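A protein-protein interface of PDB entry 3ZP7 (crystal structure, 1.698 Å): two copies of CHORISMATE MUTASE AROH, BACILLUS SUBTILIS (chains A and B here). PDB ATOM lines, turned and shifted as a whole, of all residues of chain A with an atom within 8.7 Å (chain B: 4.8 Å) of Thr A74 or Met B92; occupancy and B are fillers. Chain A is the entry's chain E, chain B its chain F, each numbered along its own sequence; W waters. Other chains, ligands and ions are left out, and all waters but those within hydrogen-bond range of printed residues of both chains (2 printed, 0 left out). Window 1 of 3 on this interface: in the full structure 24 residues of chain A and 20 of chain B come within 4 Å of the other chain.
The backbone NH (N) of Val A43 sits at hydrogen-bond distance from the backbone carbonyl oxygen (O) of Thr A94.
N of Met A45 lies within hydrogen-bond range of O of Pro A72, 2.9 Å away.
O of Leu A46 is in hydrogen-bond range of N of Met A92 (2.8 Å).
The backbone NH of Leu A47 lies within hydrogen-bond range of the backbone carbonyl oxygen of Thr A74 (3.1 Å).
O of Leu A47 lies within hydrogen-bond range of N of Met A76.
The backbone NH of Ala A59 sits close to the side-chain sulfur of Cys A75.
Among the printed residues, merely in contact across the chains: Pro A72 with Gly B5 (3.4 Å), Phe A57 with Glu B78 (3.5 Å), Pro A72 with Met B92 (3.6 Å), Gln A44 with Gly B5 (3.7 Å), Leu A46 with Leu B46 (3.7 Å), Val A73 with Met B92 (3.8 Å), Pro A72 with Arg B7 (3.8 Å), Thr A74 with Arg B7 (3.8 Å), Gln A44 with Met B92 (3.8 Å), Thr A74 with CIR B90 (3.8 Å), Met A76 with Glu B78 (3.9 Å), Thr A74 with Met B76 (3.9 Å), Thr A74 with Met B92 (3.9 Å) and Met A45 with Met B92 (3.9 Å).
Water W2 lies within hydrogen-bond range of OG1 of Thr A74 (2.5 Å), O of Cys A75 (2.7 Å) and OE2 of Glu B78 (3.3 Å).
Water W1 lies within hydrogen-bond range of OE2 of Glu B78, N of Cys A75 and OG1 of Thr A74.
N of Gly B5 is in hydrogen-bond range of O of Val A43 (3.0 Å).
The side-chain hydroxyl (OG1) of Thr B94 sits at hydrogen-bond distance from the side-chain amide oxygen (OE1) of Gln A44, 2.7 Å away.
O of Val A73 is in hydrogen-bond range of NH1 of Arg B7.
OE1 of Glu B78 sits close to O of Cys A75, 2.7 Å away.
SD of Met A76 lies close to SD of Met B76, at 3.6 Å.
Gln A44 touches Thr B94, but with the chains exchanged Thr A94 does not touch Gln B44 (7.3 Å).
Met A45 touches Met B92, but with the chains exchanged Met A92 does not touch Met B45 (13.0 Å).
Leu A46 touches its own counterpart, Leu B46.
Met B76 touches its own counterpart, Met A76.
8 positions are printed for both chains.
Of the 19 pairs that touch across the chains among the printed residues, 2 have their exchanged pair printed and touching as well.
Of the 13 printed residues of chain B, 8 touch a printed residue of chain A.
Printed residues of chain B that touch a printed residue of chain A: Gly B5, Arg B7, Leu B46, Met B76, Glu B78, CIR B90, Met B92 and Thr B94.
Printed residues of chain A that touch a printed residue of chain B: Val A43, Gln A44, Met A45, Leu A46, Phe A57, Pro A72, Val A73, Thr A74, Cys A75 and Met A76.
Hydrophobic or aromatic side chains of chain A that line the printed part of chain B: Val A43, Leu A46, Phe A57, Pro A72 and Met A76.
Among the printed residues, 19 pairs touch across the chains.
Among the printed residues, no Asp or Glu carboxylate lies within 4 Å of a Lys or Arg side-chain nitrogen of the other chain.
Printed residues of chain B within 4 Å of Phe A57: Glu B78 (3.5 Å).
Val A62 touches none of the printed residues of chain B.
Printed residues of chain B within 4 Å of Pro A72: Gly B5 (3.4 Å), Arg B7 (3.8 Å) and Met B92 (3.6 Å).
Printed residues of chain B within 4 Å of Thr A74: Arg B7, Met B76, CIR B90 and Met B92.
Of the printed residues of chain A, Leu B46 touches Leu A46.
Of the printed residues of chain A, Met B76 touches Thr A74 (3.9 Å) and Met A76 (3.6 Å).
The nearest printed residue of chain B that does not touch Thr A74 is Glu B78 (4.4 Å).
The nearest printed residue of chain B that does not touch Val A43 is Thr B94 (4.1 Å).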
ATOM      1  N   VAL A  43     -11.716  -7.141 -11.281  1.00  0.00           N
ATOM      2  CA  VAL A  43     -11.763  -7.639  -9.911  1.00  0.00           C
ATOM      3  C   VAL A  43     -11.250  -6.552  -8.983  1.00  0.00           C
ATOM      4  O   VAL A  43     -11.890  -6.191  -7.987  1.00  0.00           O
ATOM      5  CB  VAL A  43     -10.839  -8.858  -9.782  1.00  0.00           C
ATOM      6  CG1 VAL A  43     -10.698  -9.314  -8.341  1.00  0.00           C
ATOM      7  CG2 VAL A  43     -11.352  -9.991 -10.679  1.00  0.00           C
ATOM      8  N   GLN A  44     -10.084  -6.019  -9.334  1.00  0.00           N
ATOM      9  CA  GLN A  44      -9.400  -5.035  -8.495  1.00  0.00           C
ATOM     10  C   GLN A  44      -8.174  -4.535  -9.232  1.00  0.00           C
ATOM     11  O   GLN A  44      -7.784  -5.110 -10.260  1.00  0.00           O
ATOM     12  CB  GLN A  44      -8.967  -5.680  -7.184  1.00  0.00           C
ATOM     13  CG  GLN A  44      -7.834  -6.723  -7.361  1.00  0.00           C
ATOM     14  CD  GLN A  44      -7.614  -7.552  -6.117  1.00  0.00           C
ATOM     15  OE1 GLN A  44      -8.561  -7.983  -5.467  1.00  0.00           O
ATOM     16  NE2 GLN A  44      -6.353  -7.764  -5.767  1.00  0.00           N
ATOM     17  N   MET A  45      -7.570  -3.457  -8.722  1.00  0.00           N
ATOM     18  CA  MET A  45      -6.316  -2.945  -9.292  1.00  0.00           C
ATOM     19  C   MET A  45      -5.314  -2.634  -8.197  1.00  0.00           C
ATOM     20  O   MET A  45      -5.693  -2.178  -7.126  1.00  0.00           O
ATOM     21  CB  MET A  45      -6.568  -1.666 -10.107  1.00  0.00           C
ATOM     22  CG  MET A  45      -7.579  -1.830 -11.218  1.00  0.00           C
ATOM     23  SD  MET A  45      -7.466  -0.470 -12.393  1.00  0.00           S
ATOM     24  CE  MET A  45      -5.708  -0.307 -12.504  1.00  0.00           C
ATOM     25  N   LEU A  46      -4.034  -2.878  -8.465  1.00  0.00           N
ATOM     26  CA  LEU A  46      -2.963  -2.418  -7.576  1.00  0.00           C
ATOM     27  C   LEU A  46      -2.081  -1.473  -8.368  1.00  0.00           C
ATOM     28  O   LEU A  46      -1.707  -1.774  -9.505  1.00  0.00           O
ATOM     29  CB  LEU A  46      -2.109  -3.600  -7.096  1.00  0.00           C
ATOM     30  CG  LEU A  46      -2.834  -4.764  -6.423  1.00  0.00           C
ATOM     31  CD1 LEU A  46      -1.849  -5.896  -6.126  1.00  0.00           C
ATOM     32  CD2 LEU A  46      -3.546  -4.315  -5.149  1.00  0.00           C
ATOM     33  N   LEU A  47      -1.755  -0.323  -7.777  1.00  0.00           N
ATOM     34  CA  LEU A  47      -0.837   0.620  -8.397  1.00  0.00           C
ATOM     35  C   LEU A  47       0.367   0.761  -7.494  1.00  0.00           C
ATOM     36  O   LEU A  47       0.240   0.690  -6.276  1.00  0.00           O
ATOM     37  CB  LEU A  47      -1.499   1.987  -8.551  1.00  0.00           C
ATOM     38  CG  LEU A  47      -2.865   2.005  -9.256  1.00  0.00           C
ATOM     39  CD1 LEU A  47      -3.310   3.425  -9.529  1.00  0.00           C
ATOM     40  CD2 LEU A  47      -2.855   1.202 -10.531  1.00  0.00           C
ATOM     41  N   SER A  48       1.537   0.936  -8.085  1.00  0.00           N
ATOM     42  CA  SER A  48       2.724   1.158  -7.285  1.00  0.00           C
ATOM     43  C   SER A  48       3.513   2.328  -7.827  1.00  0.00           C
ATOM     44  O   SER A  48       3.405   2.680  -9.007  1.00  0.00           O
ATOM     45  CB  SER A  48       3.605  -0.093  -7.246  1.00  0.00           C
ATOM     46  OG  SER A  48       4.211  -0.331  -8.513  1.00  0.00           O
ATOM     47  N   ALA A  49       4.309   2.932  -6.954  1.00  0.00           N
ATOM     48  CA  ALA A  49       5.206   4.004  -7.364  1.00  0.00           C
ATOM     49  C   ALA A  49       6.560   3.789  -6.718  1.00  0.00           C
ATOM     50  O   ALA A  49       6.653   3.362  -5.574  1.00  0.00           O
ATOM     51  CB  ALA A  49       4.656   5.359  -6.953  1.00  0.00           C
ATOM     52  N   PHE A  57      -1.443  10.070  -4.679  1.00  0.00           N
ATOM     53  CA  PHE A  57      -1.658   8.652  -5.001  1.00  0.00           C
ATOM     54  C   PHE A  57      -2.089   8.519  -6.463  1.00  0.00           C
ATOM     55  O   PHE A  57      -3.025   9.191  -6.877  1.00  0.00           O
ATOM     56  CB  PHE A  57      -2.770   8.060  -4.127  1.00  0.00           C
ATOM     57  CG  PHE A  57      -2.380   7.836  -2.695  1.00  0.00           C
ATOM     58  CD1 PHE A  57      -1.570   6.768  -2.344  1.00  0.00           C
ATOM     59  CD2 PHE A  57      -2.845   8.683  -1.694  1.00  0.00           C
ATOM     60  CE1 PHE A  57      -1.218   6.546  -1.031  1.00  0.00           C
ATOM     61  CE2 PHE A  57      -2.491   8.472  -0.371  1.00  0.00           C
ATOM     62  CZ  PHE A  57      -1.676   7.399  -0.037  1.00  0.00           C
ATOM     63  N   PRO A  58      -1.418   7.652  -7.251  1.00  0.00           N
ATOM     64  CA  PRO A  58      -1.845   7.473  -8.648  1.00  0.00           C
ATOM     65  C   PRO A  58      -3.292   6.990  -8.763  1.00  0.00           C
ATOM     66  O   PRO A  58      -3.920   7.208  -9.808  1.00  0.00           O
ATOM     67  CB  PRO A  58      -0.892   6.398  -9.172  1.00  0.00           C
ATOM     68  CG  PRO A  58       0.339   6.551  -8.327  1.00  0.00           C
ATOM     69  CD  PRO A  58      -0.179   6.913  -6.958  1.00  0.00           C
ATOM     70  N   ALA A  59      -3.814   6.363  -7.708  1.00  0.00           N
ATOM     71  CA  ALA A  59      -5.200   5.884  -7.702  1.00  0.00           C
ATOM     72  C   ALA A  59      -6.214   6.995  -7.931  1.00  0.00           C
ATOM     73  O   ALA A  59      -7.345   6.741  -8.346  1.00  0.00           O
ATOM     74  CB  ALA A  59      -5.515   5.149  -6.389  1.00  0.00           C
ATOM     75  N   LYS A  60      -5.820   8.230  -7.648  1.00  0.00           N
ATOM     76  CA  LYS A  60      -6.715   9.360  -7.843  1.00  0.00           C
ATOM     77  C   LYS A  60      -7.114   9.511  -9.315  1.00  0.00           C
ATOM     78  O   LYS A  60      -8.188  10.046  -9.630  1.00  0.00           O
ATOM     79  CB  LYS A  60      -6.056  10.633  -7.313  1.00  0.00           C
ATOM     80  CG  LYS A  60      -6.978  11.828  -7.202  1.00  0.00           C
ATOM     81  CD  LYS A  60      -6.239  12.994  -6.553  1.00  0.00           C
ATOM     82  CE  LYS A  60      -7.111  14.233  -6.464  1.00  0.00           C
ATOM     83  NZ  LYS A  60      -6.423  15.348  -5.751  1.00  0.00           N
ATOM     84  N   VAL A  62      -7.926   7.087 -11.339  1.00  0.00           N
ATOM     85  CA  VAL A  62      -9.018   6.176 -11.653  1.00  0.00           C
ATOM     86  C   VAL A  62     -10.359   6.915 -11.624  1.00  0.00           C
ATOM     87  O   VAL A  62     -11.260   6.615 -12.404  1.00  0.00           O
ATOM     88  CB  VAL A  62      -9.021   4.967 -10.699  1.00  0.00           C
ATOM     89  CG1 VAL A  62     -10.162   3.992 -11.031  1.00  0.00           C
ATOM     90  CG2 VAL A  62      -7.689   4.264 -10.775  1.00  0.00           C
ATOM     91  N   ARG A  63     -10.467   7.925 -10.767  1.00  0.00           N
ATOM     92  CA  ARG A  63     -11.707   8.692 -10.657  1.00  0.00           C
ATOM     93  C   ARG A  63     -11.998   9.545 -11.893  1.00  0.00           C
ATOM     94  O   ARG A  63     -13.091  10.099 -12.041  1.00  0.00           O
ATOM     95  CB  ARG A  63     -11.689   9.563  -9.399  1.00  0.00           C
ATOM     96  CG  ARG A  63     -11.760   8.760  -8.106  1.00  0.00           C
ATOM     97  CD  ARG A  63     -12.869   7.714  -8.182  1.00  0.00           C
ATOM     98  NE  ARG A  63     -13.152   7.102  -6.887  1.00  0.00           N
ATOM     99  CZ  ARG A  63     -12.493   6.060  -6.392  1.00  0.00           C
ATOM    100  NH1 ARG A  63     -11.500   5.511  -7.084  1.00  0.00           N
ATOM    101  NH2 ARG A  63     -12.823   5.567  -5.203  1.00  0.00           N
ATOM    102  N   VAL A  71     -14.546   0.361  -9.046  1.00  0.00           N
ATOM    103  CA  VAL A  71     -13.411  -0.558  -9.133  1.00  0.00           C
ATOM    104  C   VAL A  71     -12.484  -0.336  -7.943  1.00  0.00           C
ATOM    105  O   VAL A  71     -11.993   0.781  -7.758  1.00  0.00           O
ATOM    106  CB  VAL A  71     -12.606  -0.304 -10.405  1.00  0.00           C
ATOM    107  CG1 VAL A  71     -11.360  -1.198 -10.424  1.00  0.00           C
ATOM    108  CG2 VAL A  71     -13.475  -0.530 -11.643  1.00  0.00           C
ATOM    109  N   PRO A  72     -12.242  -1.388  -7.134  1.00  0.00           N
ATOM    110  CA  PRO A  72     -11.422  -1.214  -5.929  1.00  0.00           C
ATOM    111  C   PRO A  72      -9.946  -1.142  -6.269  1.00  0.00           C
ATOM    112  O   PRO A  72      -9.435  -1.939  -7.065  1.00  0.00           O
ATOM    113  CB  PRO A  72     -11.742  -2.459  -5.095  1.00  0.00           C
ATOM    114  CG  PRO A  72     -12.150  -3.482  -6.085  1.00  0.00           C
ATOM    115  CD  PRO A  72     -12.824  -2.743  -7.214  1.00  0.00           C
ATOM    116  N   VAL A  73      -9.272  -0.160  -5.683  1.00  0.00           N
ATOM    117  CA  VAL A  73      -7.879   0.088  -6.000  1.00  0.00           C
ATOM    118  C   VAL A  73      -7.106   0.441  -4.733  1.00  0.00           C
ATOM    119  O   VAL A  73      -7.641   1.059  -3.811  1.00  0.00           O
ATOM    120  CB  VAL A  73      -7.751   1.202  -7.074  1.00  0.00           C
ATOM    121  CG1 VAL A  73      -8.421   2.491  -6.604  1.00  0.00           C
ATOM    122  CG2 VAL A  73      -6.286   1.441  -7.462  1.00  0.00           C
ATOM    123  N   THR A  74      -5.856   0.016  -4.668  1.00  0.00           N
ATOM    124  CA  THR A  74      -5.032   0.463  -3.565  1.00  0.00           C
ATOM    125  C   THR A  74      -3.623   0.633  -4.089  1.00  0.00           C
ATOM    126  O   THR A  74      -3.284   0.084  -5.132  1.00  0.00           O
ATOM    127  CB  THR A  74      -5.120  -0.466  -2.360  1.00  0.00           C
ATOM    128  OG1 THR A  74      -4.799   0.269  -1.170  1.00  0.00           O
ATOM    129  CG2 THR A  74      -4.200  -1.658  -2.530  1.00  0.00           C
ATOM    130  N   CYS A  75      -2.816   1.423  -3.384  1.00  0.00           N
ATOM    131  CA  CYS A  75      -1.486   1.731  -3.878  1.00  0.00           C
ATOM    132  C   CYS A  75      -0.448   1.132  -2.952  1.00  0.00           C
ATOM    133  O   CYS A  75      -0.737   0.839  -1.791  1.00  0.00           O
ATOM    134  CB  CYS A  75      -1.286   3.243  -4.005  1.00  0.00           C
ATOM    135  SG  CYS A  75      -2.512   4.018  -5.073  1.00  0.00           S
ATOM    136  N   MET A  76       0.738   0.881  -3.488  1.00  0.00           N
ATOM    137  CA  MET A  76       1.835   0.361  -2.688  1.00  0.00           C
ATOM    138  C   MET A  76       3.159   0.960  -3.135  1.00  0.00           C
ATOM    139  O   MET A  76       3.259   1.500  -4.232  1.00  0.00           O
ATOM    140  CB  MET A  76       1.885  -1.168  -2.788  1.00  0.00           C
ATOM    141  CG  MET A  76       1.984  -1.704  -4.221  1.00  0.00           C
ATOM    142  SD  MET A  76       1.250  -3.348  -4.378  1.00  0.00           S
ATOM    143  CE  MET A  76       1.862  -3.884  -5.987  1.00  0.00           C
ATOM    144  N   GLN A  77       4.174   0.852  -2.281  1.00  0.00           N
ATOM    145  CA  GLN A  77       5.505   1.330  -2.650  1.00  0.00           C
ATOM    146  C   GLN A  77       6.304   0.252  -3.372  1.00  0.00           C
ATOM    147  O   GLN A  77       6.351  -0.905  -2.955  1.00  0.00           O
ATOM    148  CB  GLN A  77       6.273   1.842  -1.431  1.00  0.00           C
ATOM    149  CG  GLN A  77       7.625   2.471  -1.783  1.00  0.00           C
ATOM    150  CD  GLN A  77       8.318   3.105  -0.593  1.00  0.00           C
ATOM    151  OE1 GLN A  77       7.876   4.130  -0.071  1.00  0.00           O
ATOM    152  NE2 GLN A  77       9.416   2.504  -0.164  1.00  0.00           N
ATOM    153  C   CIR A  90       1.649   0.062 -11.993  1.00  0.00           C
ATOM    154  O   CIR A  90       1.116   0.519 -10.954  1.00  0.00           O
ATOM    155  CA  CIR A  90       3.060   0.396 -12.358  1.00  0.00           C
ATOM    156  N   CIR A  90       3.478   1.665 -11.806  1.00  0.00           N
ATOM    157  C3  CIR A  90       3.981  -0.705 -11.915  1.00  0.00           C
ATOM    158  C4  CIR A  90       5.385  -0.601 -12.414  1.00  0.00           C
ATOM    159  C5  CIR A  90       6.377  -1.553 -11.842  1.00  0.00           C
ATOM    160  N6  CIR A  90       7.683  -1.551 -12.434  1.00  0.00           N
ATOM    161  C7  CIR A  90       8.735  -0.786 -11.843  1.00  0.00           C
ATOM    162  O7  CIR A  90       8.535  -0.121 -10.828  1.00  0.00           O
ATOM    163  N8  CIR A  90      10.034  -0.804 -12.446  1.00  0.00           N
ATOM    164  N   VAL A  91       1.006  -0.717 -12.855  1.00  0.00           N
ATOM    165  CA  VAL A  91      -0.373  -1.150 -12.661  1.00  0.00           C
ATOM    166  C   VAL A  91      -0.445  -2.655 -12.746  1.00  0.00           C
ATOM    167  O   VAL A  91       0.181  -3.250 -13.622  1.00  0.00           O
ATOM    168  CB  VAL A  91      -1.269  -0.586 -13.808  1.00  0.00           C
ATOM    169  CG1 VAL A  91      -2.628  -1.260 -13.813  1.00  0.00           C
ATOM    170  CG2 VAL A  91      -1.400   0.918 -13.688  1.00  0.00           C
ATOM    171  N   MET A  92      -1.180  -3.288 -11.825  1.00  0.00           N
ATOM    172  CA  MET A  92      -1.634  -4.659 -12.030  1.00  0.00           C
ATOM    173  C   MET A  92      -3.158  -4.670 -11.965  1.00  0.00           C
ATOM    174  O   MET A  92      -3.743  -4.523 -10.892  1.00  0.00           O
ATOM    175  CB  MET A  92      -1.048  -5.629 -10.996  1.00  0.00           C
ATOM    176  CG  MET A  92      -1.550  -7.057 -11.157  1.00  0.00           C
ATOM    177  SD  MET A  92      -0.762  -7.958 -12.507  1.00  0.00           S
ATOM    178  CE  MET A  92       0.754  -8.462 -11.672  1.00  0.00           C
ATOM    179  N   THR A  94      -6.585  -6.655 -12.505  1.00  0.00           N
ATOM    180  CA  THR A  94      -7.023  -8.048 -12.482  1.00  0.00           C
ATOM    181  C   THR A  94      -8.416  -8.133 -13.096  1.00  0.00           C
ATOM    182  O   THR A  94      -9.337  -7.484 -12.600  1.00  0.00           O
ATOM    183  CB  THR A  94      -7.025  -8.566 -11.032  1.00  0.00           C
ATOM    184  OG1 THR A  94      -5.727  -8.336 -10.457  1.00  0.00           O
ATOM    185  CG2 THR A  94      -7.344 -10.051 -10.991  1.00  0.00           C
ATOM    186  N   GLY B   5     -12.641  -7.477  -5.411  1.00  0.00           N
ATOM    187  CA  GLY B   5     -11.894  -6.930  -4.287  1.00  0.00           C
ATOM    188  C   GLY B   5     -12.802  -6.163  -3.346  1.00  0.00           C
ATOM    189  O   GLY B   5     -13.694  -5.435  -3.794  1.00  0.00           O
ATOM    190  N   ILE B   6     -12.569  -6.329  -2.045  1.00  0.00           N
ATOM    191  CA  ILE B   6     -13.260  -5.542  -1.034  1.00  0.00           C
ATOM    192  C   ILE B   6     -12.208  -4.725  -0.303  1.00  0.00           C
ATOM    193  O   ILE B   6     -11.221  -5.261   0.203  1.00  0.00           O
ATOM    194  CB  ILE B   6     -13.994  -6.416  -0.020  1.00  0.00           C
ATOM    195  CG1 ILE B   6     -14.874  -7.451  -0.727  1.00  0.00           C
ATOM    196  CG2 ILE B   6     -14.839  -5.551   0.928  1.00  0.00           C
ATOM    197  CD1 ILE B   6     -15.530  -8.436   0.238  1.00  0.00           C
ATOM    198  N   ARG B   7     -12.397  -3.419  -0.243  1.00  0.00           N
ATOM    199  CA  ARG B   7     -11.440  -2.510   0.395  1.00  0.00           C
ATOM    200  C   ARG B   7     -11.835  -2.138   1.809  1.00  0.00           C
ATOM    201  O   ARG B   7     -13.017  -1.962   2.098  1.00  0.00           O
ATOM    202  CB  ARG B   7     -11.330  -1.219  -0.412  1.00  0.00           C
ATOM    203  CG  ARG B   7     -10.521  -1.334  -1.700  1.00  0.00           C
ATOM    204  CD  ARG B   7      -9.019  -1.399  -1.411  1.00  0.00           C
ATOM    205  NE  ARG B   7      -8.707  -0.841  -0.104  1.00  0.00           N
ATOM    206  CZ  ARG B   7      -8.438   0.439   0.123  1.00  0.00           C
ATOM    207  NH1 ARG B   7      -8.423   1.312  -0.878  1.00  0.00           N
ATOM    208  NH2 ARG B   7      -8.188   0.840   1.358  1.00  0.00           N
ATOM    209  N   GLN B  44      -7.371 -14.385  -1.372  1.00  0.00           N
ATOM    210  CA  GLN B  44      -6.166 -13.898  -0.703  1.00  0.00           C
ATOM    211  C   GLN B  44      -6.467 -12.506  -0.182  1.00  0.00           C
ATOM    212  O   GLN B  44      -7.494 -11.915  -0.535  1.00  0.00           O
ATOM    213  CB  GLN B  44      -4.998 -13.812  -1.686  1.00  0.00           C
ATOM    214  CG  GLN B  44      -5.190 -12.742  -2.752  1.00  0.00           C
ATOM    215  CD  GLN B  44      -4.247 -12.908  -3.915  1.00  0.00           C
ATOM    216  OE1 GLN B  44      -3.993 -14.021  -4.366  1.00  0.00           O
ATOM    217  NE2 GLN B  44      -3.714 -11.794  -4.407  1.00  0.00           N
ATOM    218  N   MET B  45      -5.588 -11.985   0.674  1.00  0.00           N
ATOM    219  CA  MET B  45      -5.738 -10.626   1.190  1.00  0.00           C
ATOM    220  C   MET B  45      -4.406  -9.918   1.177  1.00  0.00           C
ATOM    221  O   MET B  45      -3.364 -10.541   1.390  1.00  0.00           O
ATOM    222  CB  MET B  45      -6.249 -10.645   2.632  1.00  0.00           C
ATOM    223  CG  MET B  45      -7.572 -11.330   2.810  1.00  0.00           C
ATOM    224  SD  MET B  45      -8.195 -11.101   4.482  1.00  0.00           S
ATOM    225  CE  MET B  45      -7.719  -9.398   4.760  1.00  0.00           C
ATOM    226  N   LEU B  46      -4.443  -8.612   0.928  1.00  0.00           N
ATOM    227  CA  LEU B  46      -3.255  -7.781   1.032  1.00  0.00           C
ATOM    228  C   LEU B  46      -3.533  -6.736   2.099  1.00  0.00           C
ATOM    229  O   LEU B  46      -4.586  -6.107   2.088  1.00  0.00           O
ATOM    230  CB  LEU B  46      -2.973  -7.079  -0.288  1.00  0.00           C
ATOM    231  CG  LEU B  46      -2.703  -8.000  -1.470  1.00  0.00           C
ATOM    232  CD1 LEU B  46      -2.487  -7.156  -2.707  1.00  0.00           C
ATOM    233  CD2 LEU B  46      -1.496  -8.886  -1.179  1.00  0.00           C
ATOM    234  N   MET B  76       2.306  -5.130   2.818  1.00  0.00           N
ATOM    235  CA  MET B  76       3.180  -4.292   2.021  1.00  0.00           C
ATOM    236  C   MET B  76       3.194  -2.892   2.596  1.00  0.00           C
ATOM    237  O   MET B  76       2.322  -2.530   3.387  1.00  0.00           O
ATOM    238  CB  MET B  76       2.688  -4.261   0.571  1.00  0.00           C
ATOM    239  CG  MET B  76       1.264  -3.739   0.440  1.00  0.00           C
ATOM    240  SD  MET B  76       0.395  -4.369  -1.009  1.00  0.00           S
ATOM    241  CE  MET B  76      -1.164  -3.495  -0.863  1.00  0.00           C
ATOM    242  N   GLU B  78       2.472   0.948   2.265  1.00  0.00           N
ATOM    243  CA  GLU B  78       1.729   1.921   1.488  1.00  0.00           C
ATOM    244  C   GLU B  78       2.683   2.972   0.922  1.00  0.00           C
ATOM    245  O   GLU B  78       3.694   3.318   1.528  1.00  0.00           O
ATOM    246  CB  GLU B  78       0.667   2.580   2.373  1.00  0.00           C
ATOM    247  CG  GLU B  78      -0.047   3.764   1.744  1.00  0.00           C
ATOM    248  CD  GLU B  78      -0.903   3.375   0.563  1.00  0.00           C
ATOM    249  OE1 GLU B  78      -0.347   3.179  -0.540  1.00  0.00           O
ATOM    250  OE2 GLU B  78      -2.132   3.280   0.731  1.00  0.00           O
ATOM    251  C   CIR B  90      -5.635  -2.160   4.168  1.00  0.00           C
ATOM    252  O   CIR B  90      -4.630  -2.901   4.374  1.00  0.00           O
ATOM    253  CA  CIR B  90      -5.595  -0.693   4.482  1.00  0.00           C
ATOM    254  N   CIR B  90      -4.631  -0.380   5.513  1.00  0.00           N
ATOM    255  C3  CIR B  90      -5.307   0.054   3.223  1.00  0.00           C
ATOM    256  C4  CIR B  90      -5.347   1.550   3.297  1.00  0.00           C
ATOM    257  C5  CIR B  90      -5.052   2.313   2.050  1.00  0.00           C
ATOM    258  N6  CIR B  90      -5.027   3.747   2.135  1.00  0.00           N
ATOM    259  C7  CIR B  90      -6.051   4.560   1.553  1.00  0.00           C
ATOM    260  O7  CIR B  90      -5.975   5.779   1.648  1.00  0.00           O
ATOM    261  N8  CIR B  90      -7.166   3.971   0.872  1.00  0.00           N
ATOM    262  N   VAL B  91      -6.781  -2.603   3.651  1.00  0.00           N
ATOM    263  CA  VAL B  91      -7.011  -3.997   3.310  1.00  0.00           C
ATOM    264  C   VAL B  91      -7.524  -4.089   1.883  1.00  0.00           C
ATOM    265  O   VAL B  91      -8.373  -3.298   1.484  1.00  0.00           O
ATOM    266  CB  VAL B  91      -8.116  -4.594   4.220  1.00  0.00           C
ATOM    267  CG1 VAL B  91      -8.505  -5.990   3.756  1.00  0.00           C
ATOM    268  CG2 VAL B  91      -7.675  -4.601   5.676  1.00  0.00           C
ATOM    269  N   MET B  92      -6.990  -5.032   1.107  1.00  0.00           N
ATOM    270  CA  MET B  92      -7.637  -5.465  -0.127  1.00  0.00           C
ATOM    271  C   MET B  92      -7.922  -6.946   0.034  1.00  0.00           C
ATOM    272  O   MET B  92      -7.010  -7.774  -0.044  1.00  0.00           O
ATOM    273  CB  MET B  92      -6.764  -5.228  -1.375  1.00  0.00           C
ATOM    274  CG  MET B  92      -7.454  -5.641  -2.697  1.00  0.00           C
ATOM    275  SD  MET B  92      -8.838  -4.576  -3.213  1.00  0.00           S
ATOM    276  CE  MET B  92      -7.912  -3.277  -4.049  1.00  0.00           C
ATOM    277  N   MET B  93      -9.190  -7.270   0.272  1.00  0.00           N
ATOM    278  CA  MET B  93      -9.630  -8.650   0.455  1.00  0.00           C
ATOM    279  C   MET B  93     -10.314  -9.139  -0.818  1.00  0.00           C
ATOM    280  O   MET B  93     -11.377  -8.647  -1.183  1.00  0.00           O
ATOM    281  CB  MET B  93     -10.612  -8.739   1.633  1.00  0.00           C
ATOM    282  CG  MET B  93     -11.119 -10.145   1.934  1.00  0.00           C
ATOM    283  SD  MET B  93     -12.458 -10.155   3.142  1.00  0.00           S
ATOM    284  CE  MET B  93     -11.632  -9.549   4.622  1.00  0.00           C
ATOM    285  N   THR B  94      -9.693 -10.108  -1.488  1.00  0.00           N
ATOM    286  CA  THR B  94     -10.187 -10.616  -2.766  1.00  0.00           C
ATOM    287  C   THR B  94     -11.055 -11.834  -2.515  1.00  0.00           C
ATOM    288  O   THR B  94     -10.595 -12.807  -1.940  1.00  0.00           O
ATOM    289  CB  THR B  94      -8.991 -11.026  -3.655  1.00  0.00           C
ATOM    290  OG1 THR B  94      -8.069  -9.933  -3.720  1.00  0.00           O
ATOM    291  CG2 THR B  94      -9.435 -11.373  -5.066  1.00  0.00           C
HETATM  292  O   HOH W   1      -3.876   3.472  -1.452  1.00  0.00           O
HETATM  293  O   HOH W   2      -2.611   0.120   0.053  1.00  0.00           O
